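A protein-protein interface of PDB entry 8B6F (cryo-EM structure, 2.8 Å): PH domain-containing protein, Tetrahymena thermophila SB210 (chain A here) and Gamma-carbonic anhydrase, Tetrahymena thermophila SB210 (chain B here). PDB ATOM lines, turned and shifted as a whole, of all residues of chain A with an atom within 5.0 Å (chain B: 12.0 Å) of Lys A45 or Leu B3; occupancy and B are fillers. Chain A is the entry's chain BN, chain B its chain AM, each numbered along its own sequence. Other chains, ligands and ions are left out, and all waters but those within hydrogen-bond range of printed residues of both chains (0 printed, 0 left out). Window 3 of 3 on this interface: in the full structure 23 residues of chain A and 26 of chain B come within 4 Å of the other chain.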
ATOM      1  N   LEU A  41      17.165 -12.131  21.852  1.00  0.00           N
ATOM      2  CA  LEU A  41      16.133 -11.221  22.334  1.00  0.00           C
ATOM      3  C   LEU A  41      16.607  -9.777  22.267  1.00  0.00           C
ATOM      4  O   LEU A  41      15.838  -8.878  21.908  1.00  0.00           O
ATOM      5  CB  LEU A  41      15.733 -11.586  23.764  1.00  0.00           C
ATOM      6  CG  LEU A  41      14.662 -10.698  24.405  1.00  0.00           C
ATOM      7  CD1 LEU A  41      13.349 -10.777  23.642  1.00  0.00           C
ATOM      8  CD2 LEU A  41      14.455 -11.073  25.860  1.00  0.00           C
ATOM      9  N   ARG A  42      17.872  -9.533  22.607  1.00  0.00           N
ATOM     10  CA  ARG A  42      18.407  -8.180  22.519  1.00  0.00           C
ATOM     11  C   ARG A  42      18.415  -7.685  21.079  1.00  0.00           C
ATOM     12  O   ARG A  42      18.093  -6.521  20.814  1.00  0.00           O
ATOM     13  CB  ARG A  42      19.815  -8.138  23.107  1.00  0.00           C
ATOM     14  CG  ARG A  42      20.363  -6.737  23.286  1.00  0.00           C
ATOM     15  CD  ARG A  42      21.823  -6.772  23.688  1.00  0.00           C
ATOM     16  NE  ARG A  42      22.099  -7.842  24.639  1.00  0.00           N
ATOM     17  CZ  ARG A  42      21.842  -7.778  25.938  1.00  0.00           C
ATOM     18  NH1 ARG A  42      21.302  -6.701  26.485  1.00  0.00           N
ATOM     19  NH2 ARG A  42      22.132  -8.822  26.708  1.00  0.00           N
ATOM     20  N   HIS A  43      18.789  -8.550  20.134  1.00  0.00           N
ATOM     21  CA  HIS A  43      18.778  -8.149  18.730  1.00  0.00           C
ATOM     22  C   HIS A  43      17.362  -7.846  18.261  1.00  0.00           C
ATOM     23  O   HIS A  43      17.142  -6.905  17.489  1.00  0.00           O
ATOM     24  CB  HIS A  43      19.415  -9.237  17.869  1.00  0.00           C
ATOM     25  CG  HIS A  43      20.908  -9.275  17.963  1.00  0.00           C
ATOM     26  ND1 HIS A  43      21.710  -8.254  17.500  1.00  0.00           N
ATOM     27  CD2 HIS A  43      21.746 -10.212  18.465  1.00  0.00           C
ATOM     28  CE1 HIS A  43      22.977  -8.558  17.718  1.00  0.00           C
ATOM     29  NE2 HIS A  43      23.027  -9.742  18.301  1.00  0.00           N
ATOM     30  N   ILE A  44      16.388  -8.642  18.705  1.00  0.00           N
ATOM     31  CA  ILE A  44      14.993  -8.367  18.370  1.00  0.00           C
ATOM     32  C   ILE A  44      14.569  -7.024  18.948  1.00  0.00           C
ATOM     33  O   ILE A  44      13.895  -6.230  18.282  1.00  0.00           O
ATOM     34  CB  ILE A  44      14.092  -9.513  18.867  1.00  0.00           C
ATOM     35  CG1 ILE A  44      14.382 -10.804  18.094  1.00  0.00           C
ATOM     36  CG2 ILE A  44      12.620  -9.128  18.773  1.00  0.00           C
ATOM     37  CD1 ILE A  44      13.945 -10.779  16.643  1.00  0.00           C
ATOM     38  N   LYS A  45      14.963  -6.745  20.192  1.00  0.00           N
ATOM     39  CA  LYS A  45      14.627  -5.466  20.806  1.00  0.00           C
ATOM     40  C   LYS A  45      15.238  -4.307  20.030  1.00  0.00           C
ATOM     41  O   LYS A  45      14.588  -3.277  19.826  1.00  0.00           O
ATOM     42  CB  LYS A  45      15.097  -5.438  22.261  1.00  0.00           C
ATOM     43  CG  LYS A  45      14.308  -6.340  23.192  1.00  0.00           C
ATOM     44  CD  LYS A  45      14.941  -6.375  24.571  1.00  0.00           C
ATOM     45  CE  LYS A  45      14.069  -7.121  25.563  1.00  0.00           C
ATOM     46  NZ  LYS A  45      14.746  -7.300  26.877  1.00  0.00           N
ATOM     47  N   ALA A  46      16.478  -4.465  19.571  1.00  0.00           N
ATOM     48  CA  ALA A  46      17.100  -3.426  18.760  1.00  0.00           C
ATOM     49  C   ALA A  46      16.344  -3.227  17.455  1.00  0.00           C
ATOM     50  O   ALA A  46      16.135  -2.092  17.014  1.00  0.00           O
ATOM     51  CB  ALA A  46      18.562  -3.777  18.488  1.00  0.00           C
ATOM     52  N   SER A  47      15.918  -4.322  16.824  1.00  0.00           N
ATOM     53  CA  SER A  47      15.126  -4.206  15.604  1.00  0.00           C
ATOM     54  C   SER A  47      13.801  -3.505  15.871  1.00  0.00           C
ATOM     55  O   SER A  47      13.245  -2.872  14.968  1.00  0.00           O
ATOM     56  CB  SER A  47      14.889  -5.589  14.998  1.00  0.00           C
ATOM     57  OG  SER A  47      14.150  -6.414  15.881  1.00  0.00           O
ATOM     58  N   TRP A  48      13.262  -3.632  17.085  1.00  0.00           N
ATOM     59  CA  TRP A  48      12.071  -2.870  17.450  1.00  0.00           C
ATOM     60  C   TRP A  48      12.396  -1.388  17.606  1.00  0.00           C
ATOM     61  O   TRP A  48      11.668  -0.526  17.101  1.00  0.00           O
ATOM     62  CB  TRP A  48      11.475  -3.406  18.752  1.00  0.00           C
ATOM     63  CG  TRP A  48      10.973  -4.811  18.687  1.00  0.00           C
ATOM     64  CD1 TRP A  48      10.761  -5.563  17.569  1.00  0.00           C
ATOM     65  CD2 TRP A  48      10.623  -5.641  19.800  1.00  0.00           C
ATOM     66  NE1 TRP A  48      10.300  -6.809  17.919  1.00  0.00           N
ATOM     67  CE2 TRP A  48      10.205  -6.880  19.284  1.00  0.00           C
ATOM     68  CE3 TRP A  48      10.623  -5.452  21.186  1.00  0.00           C
ATOM     69  CZ2 TRP A  48       9.794  -7.929  20.103  1.00  0.00           C
ATOM     70  CZ3 TRP A  48      10.213  -6.494  21.999  1.00  0.00           C
ATOM     71  CH2 TRP A  48       9.803  -7.717  21.456  1.00  0.00           C
ATOM     72  N   VAL A  49      13.485  -1.071  18.310  1.00  0.00           N
ATOM     73  CA  VAL A  49      13.747   0.314  18.691  1.00  0.00           C
ATOM     74  C   VAL A  49      14.129   1.154  17.477  1.00  0.00           C
ATOM     75  O   VAL A  49      13.701   2.306  17.349  1.00  0.00           O
ATOM     76  CB  VAL A  49      14.841   0.373  19.774  1.00  0.00           C
ATOM     77  CG1 VAL A  49      15.187   1.817  20.108  1.00  0.00           C
ATOM     78  CG2 VAL A  49      14.397  -0.345  21.029  1.00  0.00           C
ATOM     79  N   MET B   1      26.080   0.922  25.898  1.00  0.00           N
ATOM     80  CA  MET B   1      24.954   0.028  26.284  1.00  0.00           C
ATOM     81  C   MET B   1      24.781  -1.088  25.261  1.00  0.00           C
ATOM     82  O   MET B   1      24.963  -0.877  24.064  1.00  0.00           O
ATOM     83  CB  MET B   1      23.660   0.832  26.416  1.00  0.00           C
ATOM     84  CG  MET B   1      22.458   0.005  26.837  1.00  0.00           C
ATOM     85  SD  MET B   1      21.026   1.016  27.263  1.00  0.00           S
ATOM     86  CE  MET B   1      20.774   1.931  25.742  1.00  0.00           C
ATOM     87  N   LYS B   2      24.423  -2.280  25.743  1.00  0.00           N
ATOM     88  CA  LYS B   2      24.285  -3.425  24.850  1.00  0.00           C
ATOM     89  C   LYS B   2      23.182  -3.197  23.826  1.00  0.00           C
ATOM     90  O   LYS B   2      23.320  -3.579  22.658  1.00  0.00           O
ATOM     91  CB  LYS B   2      24.009  -4.693  25.657  1.00  0.00           C
ATOM     92  CG  LYS B   2      25.061  -5.012  26.703  1.00  0.00           C
ATOM     93  CD  LYS B   2      24.792  -6.367  27.337  1.00  0.00           C
ATOM     94  CE  LYS B   2      25.849  -6.715  28.368  1.00  0.00           C
ATOM     95  NZ  LYS B   2      25.633  -8.073  28.940  1.00  0.00           N
ATOM     96  N   LEU B   3      22.074  -2.584  24.245  1.00  0.00           N
ATOM     97  CA  LEU B   3      20.999  -2.290  23.304  1.00  0.00           C
ATOM     98  C   LEU B   3      21.472  -1.344  22.209  1.00  0.00           C
ATOM     99  O   LEU B   3      21.158  -1.544  21.031  1.00  0.00           O
ATOM    100  CB  LEU B   3      19.801  -1.697  24.043  1.00  0.00           C
ATOM    101  CG  LEU B   3      18.516  -1.561  23.222  1.00  0.00           C
ATOM    102  CD1 LEU B   3      17.944  -2.926  22.879  1.00  0.00           C
ATOM    103  CD2 LEU B   3      17.489  -0.729  23.969  1.00  0.00           C
ATOM    104  N   PHE B   4      22.228  -0.308  22.575  1.00  0.00           N
ATOM    105  CA  PHE B   4      22.753   0.605  21.565  1.00  0.00           C
ATOM    106  C   PHE B   4      23.710  -0.112  20.622  1.00  0.00           C
ATOM    107  O   PHE B   4      23.695   0.127  19.409  1.00  0.00           O
ATOM    108  CB  PHE B   4      23.447   1.792  22.231  1.00  0.00           C
ATOM    109  CG  PHE B   4      24.102   2.728  21.256  1.00  0.00           C
ATOM    110  CD1 PHE B   4      23.353   3.670  20.568  1.00  0.00           C
ATOM    111  CD2 PHE B   4      25.468   2.665  21.024  1.00  0.00           C
ATOM    112  CE1 PHE B   4      23.953   4.531  19.666  1.00  0.00           C
ATOM    113  CE2 PHE B   4      26.075   3.522  20.126  1.00  0.00           C
ATOM    114  CZ  PHE B   4      25.316   4.457  19.446  1.00  0.00           C
ATOM    115  N   GLN B   5      24.553  -0.996  21.159  1.00  0.00           N
ATOM    116  CA  GLN B   5      25.460  -1.754  20.305  1.00  0.00           C
ATOM    117  C   GLN B   5      24.686  -2.621  19.322  1.00  0.00           C
ATOM    118  O   GLN B   5      25.041  -2.703  18.142  1.00  0.00           O
ATOM    119  CB  GLN B   5      26.392  -2.611  21.160  1.00  0.00           C
ATOM    120  CG  GLN B   5      27.377  -1.802  21.985  1.00  0.00           C
ATOM    121  CD  GLN B   5      28.239  -2.673  22.873  1.00  0.00           C
ATOM    122  OE1 GLN B   5      28.054  -3.887  22.940  1.00  0.00           O
ATOM    123  NE2 GLN B   5      29.192  -2.055  23.562  1.00  0.00           N
ATOM    124  N   ALA B   6      23.629  -3.283  19.793  1.00  0.00           N
ATOM    125  CA  ALA B   6      22.817  -4.101  18.899  1.00  0.00           C
ATOM    126  C   ALA B   6      22.149  -3.243  17.833  1.00  0.00           C
ATOM    127  O   ALA B   6      22.078  -3.637  16.664  1.00  0.00           O
ATOM    128  CB  ALA B   6      21.771  -4.874  19.699  1.00  0.00           C
ATOM    129  N   MET B   7      21.646  -2.069  18.221  1.00  0.00           N
ATOM    130  CA  MET B   7      21.024  -1.175  17.250  1.00  0.00           C
ATOM    131  C   MET B   7      22.028  -0.721  16.200  1.00  0.00           C
ATOM    132  O   MET B   7      21.709  -0.664  15.007  1.00  0.00           O
ATOM    133  CB  MET B   7      20.415   0.036  17.953  1.00  0.00           C
ATOM    134  CG  MET B   7      19.175  -0.275  18.773  1.00  0.00           C
ATOM    135  SD  MET B   7      18.323   1.217  19.323  1.00  0.00           S
ATOM    136  CE  MET B   7      19.581   1.993  20.331  1.00  0.00           C
ATOM    137  N   TRP B   8      23.244  -0.377  16.626  1.00  0.00           N
ATOM    138  CA  TRP B   8      24.271   0.029  15.675  1.00  0.00           C
ATOM    139  C   TRP B   8      24.628  -1.113  14.734  1.00  0.00           C
ATOM    140  O   TRP B   8      24.809  -0.903  13.529  1.00  0.00           O
ATOM    141  CB  TRP B   8      25.510   0.522  16.419  1.00  0.00           C
ATOM    142  CG  TRP B   8      26.618   0.936  15.508  1.00  0.00           C
ATOM    143  CD1 TRP B   8      27.758   0.241  15.235  1.00  0.00           C
ATOM    144  CD2 TRP B   8      26.692   2.145  14.743  1.00  0.00           C
ATOM    145  NE1 TRP B   8      28.539   0.943  14.349  1.00  0.00           N
ATOM    146  CE2 TRP B   8      27.907   2.116  14.032  1.00  0.00           C
ATOM    147  CE3 TRP B   8      25.847   3.251  14.593  1.00  0.00           C
ATOM    148  CZ2 TRP B   8      28.300   3.148  13.182  1.00  0.00           C
ATOM    149  CZ3 TRP B   8      26.239   4.277  13.748  1.00  0.00           C
ATOM    150  CH2 TRP B   8      27.456   4.217  13.053  1.00  0.00           C
ATOM    151  N   THR B   9      24.740  -2.332  15.266  1.00  0.00           N
ATOM    152  CA  THR B   9      25.037  -3.484  14.421  1.00  0.00           C
ATOM    153  C   THR B   9      23.941  -3.697  13.386  1.00  0.00           C
ATOM    154  O   THR B   9      24.228  -3.961  12.212  1.00  0.00           O
ATOM    155  CB  THR B   9      25.207  -4.735  15.282  1.00  0.00           C
ATOM    156  OG1 THR B   9      26.236  -4.513  16.255  1.00  0.00           O
ATOM    157  CG2 THR B   9      25.584  -5.933  14.422  1.00  0.00           C
ATOM    158  N   ARG B  10      22.677  -3.608  13.802  1.00  0.00           N
ATOM    159  CA  ARG B  10      21.582  -3.765  12.854  1.00  0.00           C
ATOM    160  C   ARG B  10      21.611  -2.668  11.796  1.00  0.00           C
ATOM    161  O   ARG B  10      21.381  -2.932  10.611  1.00  0.00           O
ATOM    162  CB  ARG B  10      20.245  -3.769  13.594  1.00  0.00           C
ATOM    163  CG  ARG B  10      19.018  -3.645  12.693  1.00  0.00           C
ATOM    164  CD  ARG B  10      18.976  -4.724  11.620  1.00  0.00           C
ATOM    165  NE  ARG B  10      18.842  -6.060  12.186  1.00  0.00           N
ATOM    166  CZ  ARG B  10      18.718  -7.168  11.468  1.00  0.00           C
ATOM    167  NH1 ARG B  10      18.718  -7.140  10.146  1.00  0.00           N
ATOM    168  NH2 ARG B  10      18.583  -8.334  12.093  1.00  0.00           N
ATOM    169  N   THR B  11      21.888  -1.429  12.204  1.00  0.00           N
ATOM    170  CA  THR B  11      21.919  -0.328  11.247  1.00  0.00           C
ATOM    171  C   THR B  11      23.007  -0.538  10.201  1.00  0.00           C
ATOM    172  O   THR B  11      22.769  -0.374   8.999  1.00  0.00           O
ATOM    173  CB  THR B  11      22.134   0.996  11.981  1.00  0.00           C
ATOM    174  OG1 THR B  11      21.145   1.147  13.006  1.00  0.00           O
ATOM    175  CG2 THR B  11      22.033   2.168  11.014  1.00  0.00           C
ATOM    176  N   ILE B  12      24.212  -0.904  10.639  1.00  0.00           N
ATOM    177  CA  ILE B  12      25.311  -1.094   9.695  1.00  0.00           C
ATOM    178  C   ILE B  12      25.041  -2.296   8.799  1.00  0.00           C
ATOM    179  O   ILE B  12      25.376  -2.286   7.608  1.00  0.00           O
ATOM    180  CB  ILE B  12      26.650  -1.222  10.445  1.00  0.00           C
ATOM    181  CG1 ILE B  12      27.806  -1.287   9.446  1.00  0.00           C
ATOM    182  CG2 ILE B  12      26.650  -2.447  11.342  1.00  0.00           C
ATOM    183  CD1 ILE B  12      29.178  -1.200  10.085  1.00  0.00           C
ATOM    184  N   TYR B  53      21.438 -14.012  11.005  1.00  0.00           N
ATOM    185  CA  TYR B  53      22.006 -12.816  11.613  1.00  0.00           C
ATOM    186  C   TYR B  53      22.255 -13.093  13.089  1.00  0.00           C
ATOM    187  O   TYR B  53      21.317 -13.392  13.835  1.00  0.00           O
ATOM    188  CB  TYR B  53      21.061 -11.630  11.430  1.00  0.00           C
ATOM    189  CG  TYR B  53      21.477 -10.374  12.164  1.00  0.00           C
ATOM    190  CD1 TYR B  53      21.077 -10.139  13.472  1.00  0.00           C
ATOM    191  CD2 TYR B  53      22.242  -9.404  11.530  1.00  0.00           C
ATOM    192  CE1 TYR B  53      21.444  -8.983  14.133  1.00  0.00           C
ATOM    193  CE2 TYR B  53      22.612  -8.246  12.182  1.00  0.00           C
ATOM    194  CZ  TYR B  53      22.211  -8.042  13.482  1.00  0.00           C
ATOM    195  OH  TYR B  53      22.582  -6.890  14.131  1.00  0.00           O
ATOM    196  N   ASP B  54      23.518 -12.999  13.507  1.00  0.00           N
ATOM    197  CA  ASP B  54      23.999 -13.178  14.871  1.00  0.00           C
ATOM    198  C   ASP B  54      24.237 -14.653  15.202  1.00  0.00           C
ATOM    199  O   ASP B  54      24.762 -14.948  16.275  1.00  0.00           O
ATOM    200  CB  ASP B  54      23.051 -12.579  15.931  1.00  0.00           C
ATOM    201  CG  ASP B  54      23.604 -12.685  17.337  1.00  0.00           C
ATOM    202  OD1 ASP B  54      24.595 -11.991  17.645  1.00  0.00           O
ATOM    203  OD2 ASP B  54      23.043 -13.463  18.135  1.00  0.00           O
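Of the 14 printed residues of chain B, 6 touch a printed residue of chain A.
Among the printed residues, no Asp or Glu carboxylate lies within 4 Å of a Lys or Arg side-chain nitrogen of the other chain.
Among the printed residues, merely in contact across the chains: Val A49 with Met B7 (3.3 Å), His A43 with Tyr B53 (3.5 Å), Arg A42 with Lys B2 (3.5 Å), Ala A46 with Met B7 (3.5 Å), Ala A46 with Ala B6 (3.6 Å), Lys A45 with Leu B3 (3.8 Å) and Ala A46 with Leu B3 (3.9 Å).
OD1 of Asp B54 lies within hydrogen-bond range of NE2 of His A43, at 2.8 Å.
Of the printed residues of chain B, Lys A45 touches Leu B3.
Of chain A, only Lys A45 (3.8 Å) and Ala A46 (3.9 Å) come within 4 Å of Leu B3.
Of the printed residues of chain B, Arg A42 touches Lys B2 (3.5 Å).
No residue of chain B comes within 4 Å of Ile A44.
No residue of chain B comes within 4 Å of Ser A47.
Of the printed residues of chain B, Val A49 touches Met B7.
Of the printed residues of chain A, Tyr B53 touches His A43 (3.5 Å).
Of the printed residues of chain B, His A43 touches Tyr B53 (3.5 Å) and Asp B54 (2.8 Å).
Printed residues of chain A within 4 Å of Ala B6: Ala A46.
Met B1 touches none of the printed residues of chain A.
The nearest residue of chain B that does not touch Lys A45 is Met B7 (5.6 Å).
The nearest residue of chain A that does not touch Leu B3 is Arg A42 (4.1 Å).
The nearest printed residue of chain A that does not touch Met B7 is Ser A47 (5.5 Å).
OG1 of Thr B11 is in hydrogen-bond range of O of Met B7 (2.8 Å).
The backbone NH (N) of Arg B10 sits at hydrogen-bond distance from the side-chain hydroxyl (OH) of Tyr B53, 3.3 Å away.
O of His A43 is in hydrogen-bond range of OG of Ser A47 (3.4 Å).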
